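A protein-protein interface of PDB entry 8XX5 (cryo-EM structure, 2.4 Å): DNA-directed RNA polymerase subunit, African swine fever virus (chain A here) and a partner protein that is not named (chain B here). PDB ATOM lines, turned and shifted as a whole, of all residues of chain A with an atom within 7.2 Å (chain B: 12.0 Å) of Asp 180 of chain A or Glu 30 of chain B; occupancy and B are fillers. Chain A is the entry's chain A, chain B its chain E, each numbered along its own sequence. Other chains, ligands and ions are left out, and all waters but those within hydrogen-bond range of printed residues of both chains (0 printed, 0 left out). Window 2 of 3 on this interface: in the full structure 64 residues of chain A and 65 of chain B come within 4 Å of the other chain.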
ATOM      1  N   PRO A 105      38.889  -7.837 -16.923  1.00  0.00           N
ATOM      2  CA  PRO A 105      39.763  -7.790 -15.741  1.00  0.00           C
ATOM      3  C   PRO A 105      41.228  -7.887 -16.144  1.00  0.00           C
ATOM      4  O   PRO A 105      41.641  -8.840 -16.808  1.00  0.00           O
ATOM      5  CB  PRO A 105      39.316  -9.007 -14.923  1.00  0.00           C
ATOM      6  CG  PRO A 105      38.755  -9.945 -15.932  1.00  0.00           C
ATOM      7  CD  PRO A 105      38.128  -9.096 -16.999  1.00  0.00           C
ATOM      8  N   LEU A 109      42.108 -14.005 -13.005  1.00  0.00           N
ATOM      9  CA  LEU A 109      41.077 -14.493 -12.096  1.00  0.00           C
ATOM     10  C   LEU A 109      41.447 -15.841 -11.495  1.00  0.00           C
ATOM     11  O   LEU A 109      41.025 -16.156 -10.378  1.00  0.00           O
ATOM     12  CB  LEU A 109      39.736 -14.585 -12.822  1.00  0.00           C
ATOM     13  CG  LEU A 109      39.223 -13.285 -13.440  1.00  0.00           C
ATOM     14  CD1 LEU A 109      37.890 -13.513 -14.133  1.00  0.00           C
ATOM     15  CD2 LEU A 109      39.110 -12.194 -12.388  1.00  0.00           C
ATOM     16  N   VAL A 177      31.907  -4.093 -17.261  1.00  0.00           N
ATOM     17  CA  VAL A 177      32.275  -5.245 -16.445  1.00  0.00           C
ATOM     18  C   VAL A 177      31.181  -6.297 -16.548  1.00  0.00           C
ATOM     19  O   VAL A 177      30.001  -6.010 -16.320  1.00  0.00           O
ATOM     20  CB  VAL A 177      32.502  -4.825 -14.985  1.00  0.00           C
ATOM     21  CG1 VAL A 177      32.938  -6.016 -14.154  1.00  0.00           C
ATOM     22  CG2 VAL A 177      33.527  -3.705 -14.906  1.00  0.00           C
ATOM     23  N   THR A 178      31.569  -7.520 -16.895  1.00  0.00           N
ATOM     24  CA  THR A 178      30.617  -8.615 -16.962  1.00  0.00           C
ATOM     25  C   THR A 178      30.294  -9.131 -15.563  1.00  0.00           C
ATOM     26  O   THR A 178      31.053  -8.940 -14.610  1.00  0.00           O
ATOM     27  CB  THR A 178      31.160  -9.758 -17.820  1.00  0.00           C
ATOM     28  OG1 THR A 178      32.513 -10.040 -17.445  1.00  0.00           O
ATOM     29  CG2 THR A 178      31.117  -9.386 -19.292  1.00  0.00           C
ATOM     30  N   TYR A 179      29.140  -9.793 -15.448  1.00  0.00           N
ATOM     31  CA  TYR A 179      28.796 -10.451 -14.193  1.00  0.00           C
ATOM     32  C   TYR A 179      29.722 -11.621 -13.903  1.00  0.00           C
ATOM     33  O   TYR A 179      29.891 -12.003 -12.740  1.00  0.00           O
ATOM     34  CB  TYR A 179      27.339 -10.914 -14.216  1.00  0.00           C
ATOM     35  CG  TYR A 179      26.358  -9.814 -13.897  1.00  0.00           C
ATOM     36  CD1 TYR A 179      26.142  -9.413 -12.587  1.00  0.00           C
ATOM     37  CD2 TYR A 179      25.664  -9.161 -14.903  1.00  0.00           C
ATOM     38  CE1 TYR A 179      25.254  -8.404 -12.287  1.00  0.00           C
ATOM     39  CE2 TYR A 179      24.771  -8.150 -14.615  1.00  0.00           C
ATOM     40  CZ  TYR A 179      24.571  -7.775 -13.304  1.00  0.00           C
ATOM     41  OH  TYR A 179      23.684  -6.767 -13.008  1.00  0.00           O
ATOM     42  N   ASP A 180      30.327 -12.202 -14.940  1.00  0.00           N
ATOM     43  CA  ASP A 180      31.321 -13.247 -14.728  1.00  0.00           C
ATOM     44  C   ASP A 180      32.519 -12.707 -13.956  1.00  0.00           C
ATOM     45  O   ASP A 180      33.006 -13.345 -13.017  1.00  0.00           O
ATOM     46  CB  ASP A 180      31.758 -13.828 -16.072  1.00  0.00           C
ATOM     47  CG  ASP A 180      32.523 -15.124 -15.925  1.00  0.00           C
ATOM     48  OD1 ASP A 180      31.885 -16.165 -15.666  1.00  0.00           O
ATOM     49  OD2 ASP A 180      33.763 -15.104 -16.072  1.00  0.00           O
ATOM     50  N   THR A 181      32.996 -11.520 -14.333  1.00  0.00           N
ATOM     51  CA  THR A 181      34.095 -10.897 -13.603  1.00  0.00           C
ATOM     52  C   THR A 181      33.685 -10.558 -12.175  1.00  0.00           C
ATOM     53  O   THR A 181      34.479 -10.710 -11.240  1.00  0.00           O
ATOM     54  CB  THR A 181      34.569  -9.642 -14.336  1.00  0.00           C
ATOM     55  OG1 THR A 181      34.893  -9.974 -15.691  1.00  0.00           O
ATOM     56  CG2 THR A 181      35.795  -9.055 -13.657  1.00  0.00           C
ATOM     57  N   VAL A 182      32.448 -10.096 -11.991  1.00  0.00           N
ATOM     58  CA  VAL A 182      31.966  -9.757 -10.654  1.00  0.00           C
ATOM     59  C   VAL A 182      31.940 -10.993  -9.765  1.00  0.00           C
ATOM     60  O   VAL A 182      32.358 -10.948  -8.602  1.00  0.00           O
ATOM     61  CB  VAL A 182      30.579  -9.093 -10.744  1.00  0.00           C
ATOM     62  CG1 VAL A 182      30.016  -8.843  -9.357  1.00  0.00           C
ATOM     63  CG2 VAL A 182      30.667  -7.799 -11.525  1.00  0.00           C
ATOM     64  N   VAL A 183      31.455 -12.116 -10.296  1.00  0.00           N
ATOM     65  CA  VAL A 183      31.369 -13.335  -9.498  1.00  0.00           C
ATOM     66  C   VAL A 183      32.756 -13.899  -9.220  1.00  0.00           C
ATOM     67  O   VAL A 183      33.062 -14.297  -8.090  1.00  0.00           O
ATOM     68  CB  VAL A 183      30.466 -14.366 -10.195  1.00  0.00           C
ATOM     69  CG1 VAL A 183      30.724 -15.755  -9.641  1.00  0.00           C
ATOM     70  CG2 VAL A 183      29.006 -13.984 -10.026  1.00  0.00           C
ATOM     71  N   LYS A 184      33.621 -13.941 -10.237  1.00  0.00           N
ATOM     72  CA  LYS A 184      34.954 -14.505 -10.052  1.00  0.00           C
ATOM     73  C   LYS A 184      35.813 -13.673  -9.112  1.00  0.00           C
ATOM     74  O   LYS A 184      36.827 -14.172  -8.615  1.00  0.00           O
ATOM     75  CB  LYS A 184      35.659 -14.658 -11.400  1.00  0.00           C
ATOM     76  CG  LYS A 184      35.001 -15.657 -12.337  1.00  0.00           C
ATOM     77  CD  LYS A 184      34.509 -16.881 -11.584  1.00  0.00           C
ATOM     78  CE  LYS A 184      33.258 -17.458 -12.228  1.00  0.00           C
ATOM     79  NZ  LYS A 184      33.245 -17.251 -13.701  1.00  0.00           N
ATOM     80  N   LEU A 185      35.434 -12.424  -8.853  1.00  0.00           N
ATOM     81  CA  LEU A 185      36.138 -11.575  -7.906  1.00  0.00           C
ATOM     82  C   LEU A 185      35.510 -11.608  -6.519  1.00  0.00           C
ATOM     83  O   LEU A 185      35.847 -10.771  -5.676  1.00  0.00           O
ATOM     84  CB  LEU A 185      36.201 -10.140  -8.427  1.00  0.00           C
ATOM     85  CG  LEU A 185      37.304  -9.888  -9.457  1.00  0.00           C
ATOM     86  CD1 LEU A 185      37.242  -8.467  -9.985  1.00  0.00           C
ATOM     87  CD2 LEU A 185      38.670 -10.177  -8.859  1.00  0.00           C
ATOM     88  N   GLY A 186      34.604 -12.550  -6.267  1.00  0.00           N
ATOM     89  CA  GLY A 186      34.040 -12.734  -4.947  1.00  0.00           C
ATOM     90  C   GLY A 186      32.874 -11.838  -4.602  1.00  0.00           C
ATOM     91  O   GLY A 186      32.455 -11.821  -3.440  1.00  0.00           O
ATOM     92  N   LYS A 189      26.124 -10.867  -7.440  1.00  0.00           N
ATOM     93  CA  LYS A 189      25.533 -10.283  -8.639  1.00  0.00           C
ATOM     94  C   LYS A 189      24.739  -9.024  -8.324  1.00  0.00           C
ATOM     95  O   LYS A 189      24.484  -8.222  -9.228  1.00  0.00           O
ATOM     96  CB  LYS A 189      24.643 -11.304  -9.344  1.00  0.00           C
ATOM     97  CG  LYS A 189      25.396 -12.501  -9.897  1.00  0.00           C
ATOM     98  CD  LYS A 189      24.464 -13.668 -10.158  1.00  0.00           C
ATOM     99  CE  LYS A 189      24.821 -14.379 -11.449  1.00  0.00           C
ATOM    100  NZ  LYS A 189      24.249 -15.750 -11.501  1.00  0.00           N
ATOM    101  N   HIS A 192      27.239  -5.498  -8.503  1.00  0.00           N
ATOM    102  CA  HIS A 192      27.893  -5.094  -9.735  1.00  0.00           C
ATOM    103  C   HIS A 192      28.373  -3.649  -9.612  1.00  0.00           C
ATOM    104  O   HIS A 192      27.655  -2.802  -9.075  1.00  0.00           O
ATOM    105  CB  HIS A 192      26.939  -5.237 -10.920  1.00  0.00           C
ATOM    106  CG  HIS A 192      27.623  -5.235 -12.251  1.00  0.00           C
ATOM    107  ND1 HIS A 192      28.076  -4.082 -12.855  1.00  0.00           N
ATOM    108  CD2 HIS A 192      27.930  -6.247 -13.096  1.00  0.00           C
ATOM    109  CE1 HIS A 192      28.632  -4.383 -14.014  1.00  0.00           C
ATOM    110  NE2 HIS A 192      28.556  -5.691 -14.185  1.00  0.00           N
ATOM    111  N   GLU B  30      28.962 -20.533 -16.582  1.00  0.00           N
ATOM    112  CA  GLU B  30      28.506 -19.583 -17.590  1.00  0.00           C
ATOM    113  C   GLU B  30      28.351 -18.191 -16.994  1.00  0.00           C
ATOM    114  O   GLU B  30      28.938 -17.228 -17.489  1.00  0.00           O
ATOM    115  CB  GLU B  30      27.182 -20.043 -18.203  1.00  0.00           C
ATOM    116  CG  GLU B  30      26.752 -19.246 -19.423  1.00  0.00           C
ATOM    117  CD  GLU B  30      27.913 -18.906 -20.335  1.00  0.00           C
ATOM    118  OE1 GLU B  30      28.342 -19.790 -21.108  1.00  0.00           O
ATOM    119  OE2 GLU B  30      28.395 -17.754 -20.287  1.00  0.00           O
ATOM    120  N   ILE B  31      27.550 -18.106 -15.931  1.00  0.00           N
ATOM    121  CA  ILE B  31      27.310 -16.876 -15.185  1.00  0.00           C
ATOM    122  C   ILE B  31      26.640 -15.840 -16.080  1.00  0.00           C
ATOM    123  O   ILE B  31      27.304 -15.134 -16.846  1.00  0.00           O
ATOM    124  CB  ILE B  31      28.609 -16.325 -14.569  1.00  0.00           C
ATOM    125  CG1 ILE B  31      29.313 -17.424 -13.769  1.00  0.00           C
ATOM    126  CG2 ILE B  31      28.314 -15.109 -13.703  1.00  0.00           C
ATOM    127  CD1 ILE B  31      28.990 -17.425 -12.294  1.00  0.00           C
ATOM    128  N   VAL B  32      25.321 -15.742 -15.976  1.00  0.00           N
ATOM    129  CA  VAL B  32      24.541 -14.818 -16.771  1.00  0.00           C
ATOM    130  C   VAL B  32      24.130 -13.655 -15.873  1.00  0.00           C
ATOM    131  O   VAL B  32      24.421 -13.634 -14.679  1.00  0.00           O
ATOM    132  CB  VAL B  32      23.318 -15.515 -17.421  1.00  0.00           C
ATOM    133  CG1 VAL B  32      22.827 -14.745 -18.644  1.00  0.00           C
ATOM    134  CG2 VAL B  32      23.667 -16.946 -17.795  1.00  0.00           C
ATOM    135  N   GLU B  33      23.464 -12.658 -16.459  1.00  0.00           N
ATOM    136  CA  GLU B  33      23.127 -11.425 -15.753  1.00  0.00           C
ATOM    137  C   GLU B  33      22.372 -11.703 -14.461  1.00  0.00           C
ATOM    138  O   GLU B  33      22.894 -11.463 -13.368  1.00  0.00           O
ATOM    139  CB  GLU B  33      22.280 -10.519 -16.650  1.00  0.00           C
ATOM    140  CG  GLU B  33      22.583 -10.635 -18.137  1.00  0.00           C
ATOM    141  CD  GLU B  33      23.682  -9.693 -18.589  1.00  0.00           C
ATOM    142  OE1 GLU B  33      24.590  -9.406 -17.784  1.00  0.00           O
ATOM    143  OE2 GLU B  33      23.634  -9.238 -19.752  1.00  0.00           O
ATOM    144  N   SER B  34      21.156 -12.227 -14.579  1.00  0.00           N
ATOM    145  CA  SER B  34      20.363 -12.670 -13.440  1.00  0.00           C
ATOM    146  C   SER B  34      19.111 -13.372 -13.945  1.00  0.00           C
ATOM    147  O   SER B  34      18.456 -12.880 -14.872  1.00  0.00           O
ATOM    148  CB  SER B  34      19.983 -11.495 -12.536  1.00  0.00           C
ATOM    149  OG  SER B  34      21.060 -11.139 -11.688  1.00  0.00           O
ATOM    150  N   PRO B  35      18.747 -14.512 -13.375  1.00  0.00           N
ATOM    151  CA  PRO B  35      17.460 -15.122 -13.722  1.00  0.00           C
ATOM    152  C   PRO B  35      16.352 -14.601 -12.826  1.00  0.00           C
ATOM    153  O   PRO B  35      16.602 -13.791 -11.928  1.00  0.00           O
ATOM    154  CB  PRO B  35      17.705 -16.624 -13.511  1.00  0.00           C
ATOM    155  CG  PRO B  35      19.117 -16.748 -12.937  1.00  0.00           C
ATOM    156  CD  PRO B  35      19.544 -15.384 -12.502  1.00  0.00           C
ATOM    157  N   CYS B  38      17.418 -16.698  -8.985  1.00  0.00           N
ATOM    158  CA  CYS B  38      18.526 -16.342  -8.103  1.00  0.00           C
ATOM    159  C   CYS B  38      18.363 -14.924  -7.574  1.00  0.00           C
ATOM    160  O   CYS B  38      18.458 -14.687  -6.364  1.00  0.00           O
ATOM    161  CB  CYS B  38      19.856 -16.497  -8.844  1.00  0.00           C
ATOM    162  SG  CYS B  38      21.251 -16.949  -7.785  1.00  0.00           S
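The side-chain carboxylate (OD1) of Asp 180 of chain A lies within salt-bridge range of the side-chain amino group (NZ) of Lys 184 of chain A.
Tyr 179 of chain A touches Ile 31 of chain B (O to CG2, 3.6 Å).
Glu 33 of chain B touches Tyr 179 of chain A (OE1 to CD2, 3.1 Å).
Glu 30 of chain B touches Asp 180 of chain A (O to OD1, 3.6 Å).
Ile 31 of chain B touches Asp 180 of chain A.
CG1 of Val 183 of chain A touches CD1 of Ile 31 of chain B, 3.6 Å away.
Ile 31 of chain B touches Lys 184 of chain A (CG1 to NZ, 3.9 Å).
Lys 189 of chain A touches Val 32 of chain B.
O of Glu 33 of chain B touches CE of Lys 189 of chain A, at 3.99 Å.
Thr 178 of chain A touches none of the printed residues of chain B.
Of the printed residues of chain B, Tyr 179 of chain A touches Ile 31 (3.6 Å) and Glu 33 (3.1 Å).
Of chain B, only Glu 30 and Ile 31 come within 4 Å of Asp 180 of chain A.
No residue of chain B comes within 4 Å of Thr 181 of chain A.
No residue of chain B comes within 4 Å of Val 182 of chain A.
Printed residues of chain B within 4 Å of Lys 189 of chain A: Val 32 and Glu 33.
Of the printed residues of chain A, Glu 30 of chain B touches Asp 180.
Of the printed residues of chain A, Val 32 of chain B touches Lys 189.
Of the printed residues of chain A, Glu 33 of chain B touches Tyr 179 and Lys 189.
Pro 35 of chain B touches none of the printed residues of chain A.
The nearest residue of chain B that does not touch Asp 180 of chain A is Val 32 of chain B (6.1 Å).
The nearest printed residue of chain B that does not touch Tyr 179 of chain A is Val 32 of chain B (4.02 Å).
Printed residues of chain A that touch a printed residue of chain B: Tyr 179, Asp 180, Val 183, Lys 184 and Lys 189.
Hydrophobic or aromatic side chains of chain A that line the printed part of chain B: Tyr 179 and Val 183.
Printed residues of chain B that touch a printed residue of chain A: Glu 30, Ile 31, Val 32 and Glu 33.
Hydrophobic or aromatic side chains of chain B that line the printed part of chain A: Ile 31.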
